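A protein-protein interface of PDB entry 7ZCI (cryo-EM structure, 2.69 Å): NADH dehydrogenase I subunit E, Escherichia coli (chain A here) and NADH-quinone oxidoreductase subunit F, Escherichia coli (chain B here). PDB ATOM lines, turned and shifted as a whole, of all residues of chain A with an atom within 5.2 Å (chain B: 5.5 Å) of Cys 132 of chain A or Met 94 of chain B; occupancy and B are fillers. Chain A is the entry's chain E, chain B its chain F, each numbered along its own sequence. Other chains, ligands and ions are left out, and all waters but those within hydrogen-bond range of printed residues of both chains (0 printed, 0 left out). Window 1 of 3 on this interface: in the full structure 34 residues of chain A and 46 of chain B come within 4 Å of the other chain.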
ATOM      1  N   CYS A  92      24.269  24.298  22.879  1.00  0.00           N
ATOM      2  CA  CYS A  92      23.662  22.990  22.715  1.00  0.00           C
ATOM      3  C   CYS A  92      22.145  23.073  22.761  1.00  0.00           C
ATOM      4  O   CYS A  92      21.563  23.761  23.601  1.00  0.00           O
ATOM      5  CB  CYS A  92      24.153  22.030  23.783  1.00  0.00           C
ATOM      6  SG  CYS A  92      23.489  20.400  23.541  1.00  0.00           S
ATOM      7  N   ASP A  93      21.510  22.333  21.860  1.00  0.00           N
ATOM      8  CA  ASP A  93      20.072  22.354  21.664  1.00  0.00           C
ATOM      9  C   ASP A  93      19.387  21.097  22.165  1.00  0.00           C
ATOM     10  O   ASP A  93      18.159  21.077  22.262  1.00  0.00           O
ATOM     11  CB  ASP A  93      19.766  22.515  20.167  1.00  0.00           C
ATOM     12  CG  ASP A  93      18.702  23.525  19.890  1.00  0.00           C
ATOM     13  OD1 ASP A  93      18.508  24.419  20.724  1.00  0.00           O
ATOM     14  OD2 ASP A  93      18.070  23.434  18.820  1.00  0.00           O
ATOM     15  N   SER A  94      20.146  20.057  22.487  1.00  0.00           N
ATOM     16  CA  SER A  94      19.603  18.718  22.647  1.00  0.00           C
ATOM     17  C   SER A  94      18.994  18.536  24.035  1.00  0.00           C
ATOM     18  O   SER A  94      18.822  19.484  24.801  1.00  0.00           O
ATOM     19  CB  SER A  94      20.677  17.682  22.347  1.00  0.00           C
ATOM     20  OG  SER A  94      21.100  17.777  21.004  1.00  0.00           O
ATOM     21  N   PRO A 130      22.433  27.217  17.123  1.00  0.00           N
ATOM     22  CA  PRO A 130      22.149  26.014  17.911  1.00  0.00           C
ATOM     23  C   PRO A 130      22.858  24.824  17.286  1.00  0.00           C
ATOM     24  O   PRO A 130      22.736  24.569  16.088  1.00  0.00           O
ATOM     25  CB  PRO A 130      20.626  25.881  17.814  1.00  0.00           C
ATOM     26  CG  PRO A 130      20.271  26.551  16.539  1.00  0.00           C
ATOM     27  CD  PRO A 130      21.313  27.585  16.241  1.00  0.00           C
ATOM     28  N   THR A 131      23.632  24.120  18.087  1.00  0.00           N
ATOM     29  CA  THR A 131      24.244  22.879  17.654  1.00  0.00           C
ATOM     30  C   THR A 131      23.544  21.707  18.323  1.00  0.00           C
ATOM     31  O   THR A 131      22.775  21.867  19.268  1.00  0.00           O
ATOM     32  CB  THR A 131      25.742  22.874  17.974  1.00  0.00           C
ATOM     33  OG1 THR A 131      26.321  21.648  17.520  1.00  0.00           O
ATOM     34  CG2 THR A 131      25.972  23.011  19.459  1.00  0.00           C
ATOM     35  N   CYS A 132      23.847  20.510  17.841  1.00  0.00           N
ATOM     36  CA  CYS A 132      23.352  19.293  18.463  1.00  0.00           C
ATOM     37  C   CYS A 132      24.146  19.038  19.742  1.00  0.00           C
ATOM     38  O   CYS A 132      24.898  19.893  20.218  1.00  0.00           O
ATOM     39  CB  CYS A 132      23.440  18.122  17.490  1.00  0.00           C
ATOM     40  SG  CYS A 132      24.884  18.167  16.417  1.00  0.00           S
ATOM     41  N   CYS A 133      23.979  17.857  20.323  1.00  0.00           N
ATOM     42  CA  CYS A 133      24.589  17.559  21.610  1.00  0.00           C
ATOM     43  C   CYS A 133      26.109  17.562  21.518  1.00  0.00           C
ATOM     44  O   CYS A 133      26.695  16.905  20.655  1.00  0.00           O
ATOM     45  CB  CYS A 133      24.091  16.213  22.109  1.00  0.00           C
ATOM     46  SG  CYS A 133      25.155  15.441  23.302  1.00  0.00           S
ATOM     47  N   LEU A 134      26.741  18.307  22.419  1.00  0.00           N
ATOM     48  CA  LEU A 134      28.179  18.510  22.416  1.00  0.00           C
ATOM     49  C   LEU A 134      28.926  17.415  23.151  1.00  0.00           C
ATOM     50  O   LEU A 134      30.125  17.563  23.399  1.00  0.00           O
ATOM     51  CB  LEU A 134      28.516  19.870  23.026  1.00  0.00           C
ATOM     52  CG  LEU A 134      28.074  21.059  22.177  1.00  0.00           C
ATOM     53  CD1 LEU A 134      28.114  22.346  22.970  1.00  0.00           C
ATOM     54  CD2 LEU A 134      28.951  21.164  20.948  1.00  0.00           C
ATOM     55  N   ASP B  92      32.502   9.154  16.577  1.00  0.00           N
ATOM     56  CA  ASP B  92      31.547  10.223  16.325  1.00  0.00           C
ATOM     57  C   ASP B  92      30.816  10.609  17.602  1.00  0.00           C
ATOM     58  O   ASP B  92      30.949  11.737  18.081  1.00  0.00           O
ATOM     59  CB  ASP B  92      30.560   9.808  15.237  1.00  0.00           C
ATOM     60  CG  ASP B  92      30.170  10.963  14.348  1.00  0.00           C
ATOM     61  OD1 ASP B  92      30.984  11.896  14.208  1.00  0.00           O
ATOM     62  OD2 ASP B  92      29.049  10.956  13.805  1.00  0.00           O
ATOM     63  N   GLU B  93      30.062   9.671  18.178  1.00  0.00           N
ATOM     64  CA  GLU B  93      29.374   9.815  19.465  1.00  0.00           C
ATOM     65  C   GLU B  93      28.505  11.075  19.508  1.00  0.00           C
ATOM     66  O   GLU B  93      28.752  12.017  20.256  1.00  0.00           O
ATOM     67  CB  GLU B  93      30.369   9.808  20.626  1.00  0.00           C
ATOM     68  CG  GLU B  93      29.733   9.430  21.950  1.00  0.00           C
ATOM     69  CD  GLU B  93      30.492   9.967  23.137  1.00  0.00           C
ATOM     70  OE1 GLU B  93      30.924  11.133  23.090  1.00  0.00           O
ATOM     71  OE2 GLU B  93      30.651   9.227  24.123  1.00  0.00           O
ATOM     72  N   MET B  94      27.488  11.075  18.657  1.00  0.00           N
ATOM     73  CA  MET B  94      26.636  12.237  18.485  1.00  0.00           C
ATOM     74  C   MET B  94      25.277  12.088  19.145  1.00  0.00           C
ATOM     75  O   MET B  94      24.481  13.030  19.094  1.00  0.00           O
ATOM     76  CB  MET B  94      26.457  12.531  16.997  1.00  0.00           C
ATOM     77  CG  MET B  94      27.459  13.505  16.438  1.00  0.00           C
ATOM     78  SD  MET B  94      26.906  15.204  16.525  1.00  0.00           S
ATOM     79  CE  MET B  94      27.934  15.917  15.254  1.00  0.00           C
ATOM     80  N   GLU B  95      24.989  10.946  19.754  1.00  0.00           N
ATOM     81  CA  GLU B  95      23.690  10.745  20.382  1.00  0.00           C
ATOM     82  C   GLU B  95      23.544  11.652  21.596  1.00  0.00           C
ATOM     83  O   GLU B  95      24.447  11.698  22.437  1.00  0.00           O
ATOM     84  CB  GLU B  95      23.505   9.297  20.802  1.00  0.00           C
ATOM     85  CG  GLU B  95      22.149   8.974  21.402  1.00  0.00           C
ATOM     86  CD  GLU B  95      21.162   8.420  20.392  1.00  0.00           C
ATOM     87  OE1 GLU B  95      21.144   8.898  19.244  1.00  0.00           O
ATOM     88  OE2 GLU B  95      20.406   7.495  20.741  1.00  0.00           O
ATOM     89  N   PRO B  96      22.449  12.399  21.706  1.00  0.00           N
ATOM     90  CA  PRO B  96      22.234  13.227  22.894  1.00  0.00           C
ATOM     91  C   PRO B  96      22.101  12.372  24.142  1.00  0.00           C
ATOM     92  O   PRO B  96      21.288  11.450  24.200  1.00  0.00           O
ATOM     93  CB  PRO B  96      20.938  13.975  22.572  1.00  0.00           C
ATOM     94  CG  PRO B  96      20.850  13.953  21.092  1.00  0.00           C
ATOM     95  CD  PRO B  96      21.442  12.653  20.668  1.00  0.00           C
ATOM     96  N   ARG B 133      34.459  13.133  15.856  1.00  0.00           N
ATOM     97  CA  ARG B 133      33.593  14.283  15.634  1.00  0.00           C
ATOM     98  C   ARG B 133      34.386  15.577  15.770  1.00  0.00           C
ATOM     99  O   ARG B 133      35.379  15.653  16.497  1.00  0.00           O
ATOM    100  CB  ARG B 133      32.402  14.275  16.594  1.00  0.00           C
ATOM    101  CG  ARG B 133      32.717  14.669  18.019  1.00  0.00           C
ATOM    102  CD  ARG B 133      31.472  14.749  18.878  1.00  0.00           C
ATOM    103  NE  ARG B 133      30.611  15.881  18.561  1.00  0.00           N
ATOM    104  CZ  ARG B 133      29.438  16.098  19.137  1.00  0.00           C
ATOM    105  NH1 ARG B 133      28.945  15.258  20.029  1.00  0.00           N
ATOM    106  NH2 ARG B 133      28.743  17.181  18.809  1.00  0.00           N
ATOM    107  N   GLU B 135      33.841  18.416  17.116  1.00  0.00           N
ATOM    108  CA  GLU B 135      33.707  19.238  18.307  1.00  0.00           C
ATOM    109  C   GLU B 135      34.595  18.768  19.445  1.00  0.00           C
ATOM    110  O   GLU B 135      34.759  19.498  20.427  1.00  0.00           O
ATOM    111  CB  GLU B 135      32.243  19.259  18.754  1.00  0.00           C
ATOM    112  CG  GLU B 135      31.326  20.004  17.791  1.00  0.00           C
ATOM    113  CD  GLU B 135      30.879  19.151  16.619  1.00  0.00           C
ATOM    114  OE1 GLU B 135      31.000  17.913  16.699  1.00  0.00           O
ATOM    115  OE2 GLU B 135      30.427  19.718  15.606  1.00  0.00           O
ATOM    116  N   GLY B 176      30.282  17.580  11.571  1.00  0.00           N
ATOM    117  CA  GLY B 176      29.043  17.809  12.286  1.00  0.00           C
ATOM    118  C   GLY B 176      27.731  17.331  11.695  1.00  0.00           C
ATOM    119  O   GLY B 176      26.870  18.148  11.367  1.00  0.00           O
ATOM    120  N   ARG B 177      27.551  16.023  11.559  1.00  0.00           N
ATOM    121  CA  ARG B 177      26.233  15.456  11.316  1.00  0.00           C
ATOM    122  C   ARG B 177      26.068  14.224  12.192  1.00  0.00           C
ATOM    123  O   ARG B 177      27.026  13.479  12.408  1.00  0.00           O
ATOM    124  CB  ARG B 177      26.022  15.089   9.845  1.00  0.00           C
ATOM    125  CG  ARG B 177      25.629  16.251   8.966  1.00  0.00           C
ATOM    126  CD  ARG B 177      24.321  16.865   9.397  1.00  0.00           C
ATOM    127  NE  ARG B 177      23.970  18.006   8.565  1.00  0.00           N
ATOM    128  CZ  ARG B 177      23.061  18.915   8.887  1.00  0.00           C
ATOM    129  NH1 ARG B 177      22.390  18.848  10.023  1.00  0.00           N
ATOM    130  NH2 ARG B 177      22.823  19.918   8.049  1.00  0.00           N
ATOM    131  N   TYR B 178      24.855  14.024  12.700  1.00  0.00           N
ATOM    132  CA  TYR B 178      24.585  12.888  13.575  1.00  0.00           C
ATOM    133  C   TYR B 178      24.534  11.581  12.800  1.00  0.00           C
ATOM    134  O   TYR B 178      24.826  10.518  13.358  1.00  0.00           O
ATOM    135  CB  TYR B 178      23.278  13.135  14.324  1.00  0.00           C
ATOM    136  CG  TYR B 178      22.634  11.939  14.978  1.00  0.00           C
ATOM    137  CD1 TYR B 178      23.111  11.433  16.175  1.00  0.00           C
ATOM    138  CD2 TYR B 178      21.529  11.331  14.406  1.00  0.00           C
ATOM    139  CE1 TYR B 178      22.515  10.354  16.773  1.00  0.00           C
ATOM    140  CE2 TYR B 178      20.931  10.254  15.000  1.00  0.00           C
ATOM    141  CZ  TYR B 178      21.422   9.770  16.180  1.00  0.00           C
ATOM    142  OH  TYR B 178      20.810   8.693  16.765  1.00  0.00           O
ATOM    143  N   PHE B 345      15.511  17.493  16.998  1.00  0.00           N
ATOM    144  CA  PHE B 345      16.858  17.002  16.721  1.00  0.00           C
ATOM    145  C   PHE B 345      16.840  15.910  15.660  1.00  0.00           C
ATOM    146  O   PHE B 345      17.611  15.954  14.695  1.00  0.00           O
ATOM    147  CB  PHE B 345      17.501  16.479  18.003  1.00  0.00           C
ATOM    148  CG  PHE B 345      18.667  15.562  17.765  1.00  0.00           C
ATOM    149  CD1 PHE B 345      19.902  16.074  17.423  1.00  0.00           C
ATOM    150  CD2 PHE B 345      18.529  14.187  17.887  1.00  0.00           C
ATOM    151  CE1 PHE B 345      20.972  15.242  17.214  1.00  0.00           C
ATOM    152  CE2 PHE B 345      19.595  13.351  17.662  1.00  0.00           C
ATOM    153  CZ  PHE B 345      20.819  13.881  17.333  1.00  0.00           C
ATOM    154  N   ARG B 348      15.895  17.266  12.108  1.00  0.00           N
ATOM    155  CA  ARG B 348      16.921  18.045  11.433  1.00  0.00           C
ATOM    156  C   ARG B 348      18.233  17.288  11.282  1.00  0.00           C
ATOM    157  O   ARG B 348      19.134  17.782  10.602  1.00  0.00           O
ATOM    158  CB  ARG B 348      17.148  19.367  12.156  1.00  0.00           C
ATOM    159  CG  ARG B 348      18.026  19.302  13.372  1.00  0.00           C
ATOM    160  CD  ARG B 348      18.327  20.702  13.844  1.00  0.00           C
ATOM    161  NE  ARG B 348      18.530  20.773  15.283  1.00  0.00           N
ATOM    162  CZ  ARG B 348      19.703  20.611  15.875  1.00  0.00           C
ATOM    163  NH1 ARG B 348      20.795  20.337  15.182  1.00  0.00           N
ATOM    164  NH2 ARG B 348      19.783  20.728  17.195  1.00  0.00           N
ATOM    165  N   GLU B 349      18.367  16.112  11.883  1.00  0.00           N
ATOM    166  CA  GLU B 349      19.535  15.276  11.663  1.00  0.00           C
ATOM    167  C   GLU B 349      19.256  14.131  10.705  1.00  0.00           C
ATOM    168  O   GLU B 349      20.083  13.228  10.574  1.00  0.00           O
ATOM    169  CB  GLU B 349      20.066  14.746  12.991  1.00  0.00           C
ATOM    170  CG  GLU B 349      20.808  15.805  13.769  1.00  0.00           C
ATOM    171  CD  GLU B 349      21.934  16.427  12.971  1.00  0.00           C
ATOM    172  OE1 GLU B 349      22.728  15.679  12.371  1.00  0.00           O
ATOM    173  OE2 GLU B 349      22.021  17.670  12.935  1.00  0.00           O
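The side-chain carboxylate of Asp 93 of chain A is in salt-bridge range of the guanidinium group of Arg 348 of chain B, 3.6 Å away. The backbone carbonyl oxygen of Cys 133 of chain A is in hydrogen-bond range of the guanidinium group of Arg 133 of chain B (2.8 Å). SD of Met 94 of chain B sits at hydrogen-bond distance from SG of Cys 132 of chain A, 3.6 Å away.
OH of Tyr 178 of chain B sits at hydrogen-bond distance from OE1 of Glu 95 of chain B. O of Glu 93 of chain B sits at hydrogen-bond distance from NH1 of Arg 133 of chain B (3.3 Å). NE of Arg 133 of chain B lies within salt-bridge range of OE1 of Glu 135 of chain B. The guanidinium group (NH1) of Arg 348 of chain B lies within salt-bridge range of the side-chain carboxylate (OE2) of Glu 349 of chain B, 3.7 Å away. The backbone NH (N) of Asp 93 of chain A sits at hydrogen-bond distance from the backbone carbonyl oxygen (O) of Thr 131 of chain A (2.9 Å). The side-chain hydroxyl (OG) of Ser 94 of chain A sits at hydrogen-bond distance from the backbone NH (N) of Cys 133 of chain A, at 3.0 Å.
Hydrophobic or aromatic side chains of chain B that line the printed part of chain A: Met 94, Pro 96 and Phe 345. Of the 8 printed residues of chain A, 6 touch a printed residue of chain B. Along chain A the printed residues that touch a printed residue of chain B span positions 93 to 134. Among the printed residues, 9 pairs touch across the chains.
Of chain B, only Met 94 (3.6 Å) and Phe 345 (3.8 Å) come within 4 Å of Cys 132 of chain A. Of the printed residues of chain A, Met 94 of chain B touches Cys 132 (3.6 Å). Printed residues of chain A within 4 Å of Arg 348 of chain B: Asp 93 and Thr 131. Of the printed residues of chain B, Ser 94 of chain A touches Pro 96. Printed residues of chain B within 4 Å of Leu 134 of chain A: Arg 133 (3.8 Å). Of the printed residues of chain A, Phe 345 of chain B touches Cys 132. Of the printed residues of chain A, Arg 133 of chain B touches Cys 133 and Leu 134. Asp 92 of chain B touches none of the printed residues of chain A. Glu 135 of chain B touches none of the printed residues of chain A. The nearest residue of chain B that does not touch Cys 132 of chain A is Arg 348 of chain B (4.1 Å). The nearest residue of chain A that does not touch Met 94 of chain B is Cys 133 of chain A (4.4 Å).
Among the printed residues, merely in contact across the chains: Cys 133 of chain A with Pro 96 of chain B, Ser 94 of chain A with Pro 96 of chain B, Leu 134 of chain A with Arg 133 of chain B, Cys 132 of chain A with Phe 345 of chain B, Thr 131 of chain A with Arg 348 of chain B and Cys 133 of chain A with Glu 95 of chain B.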
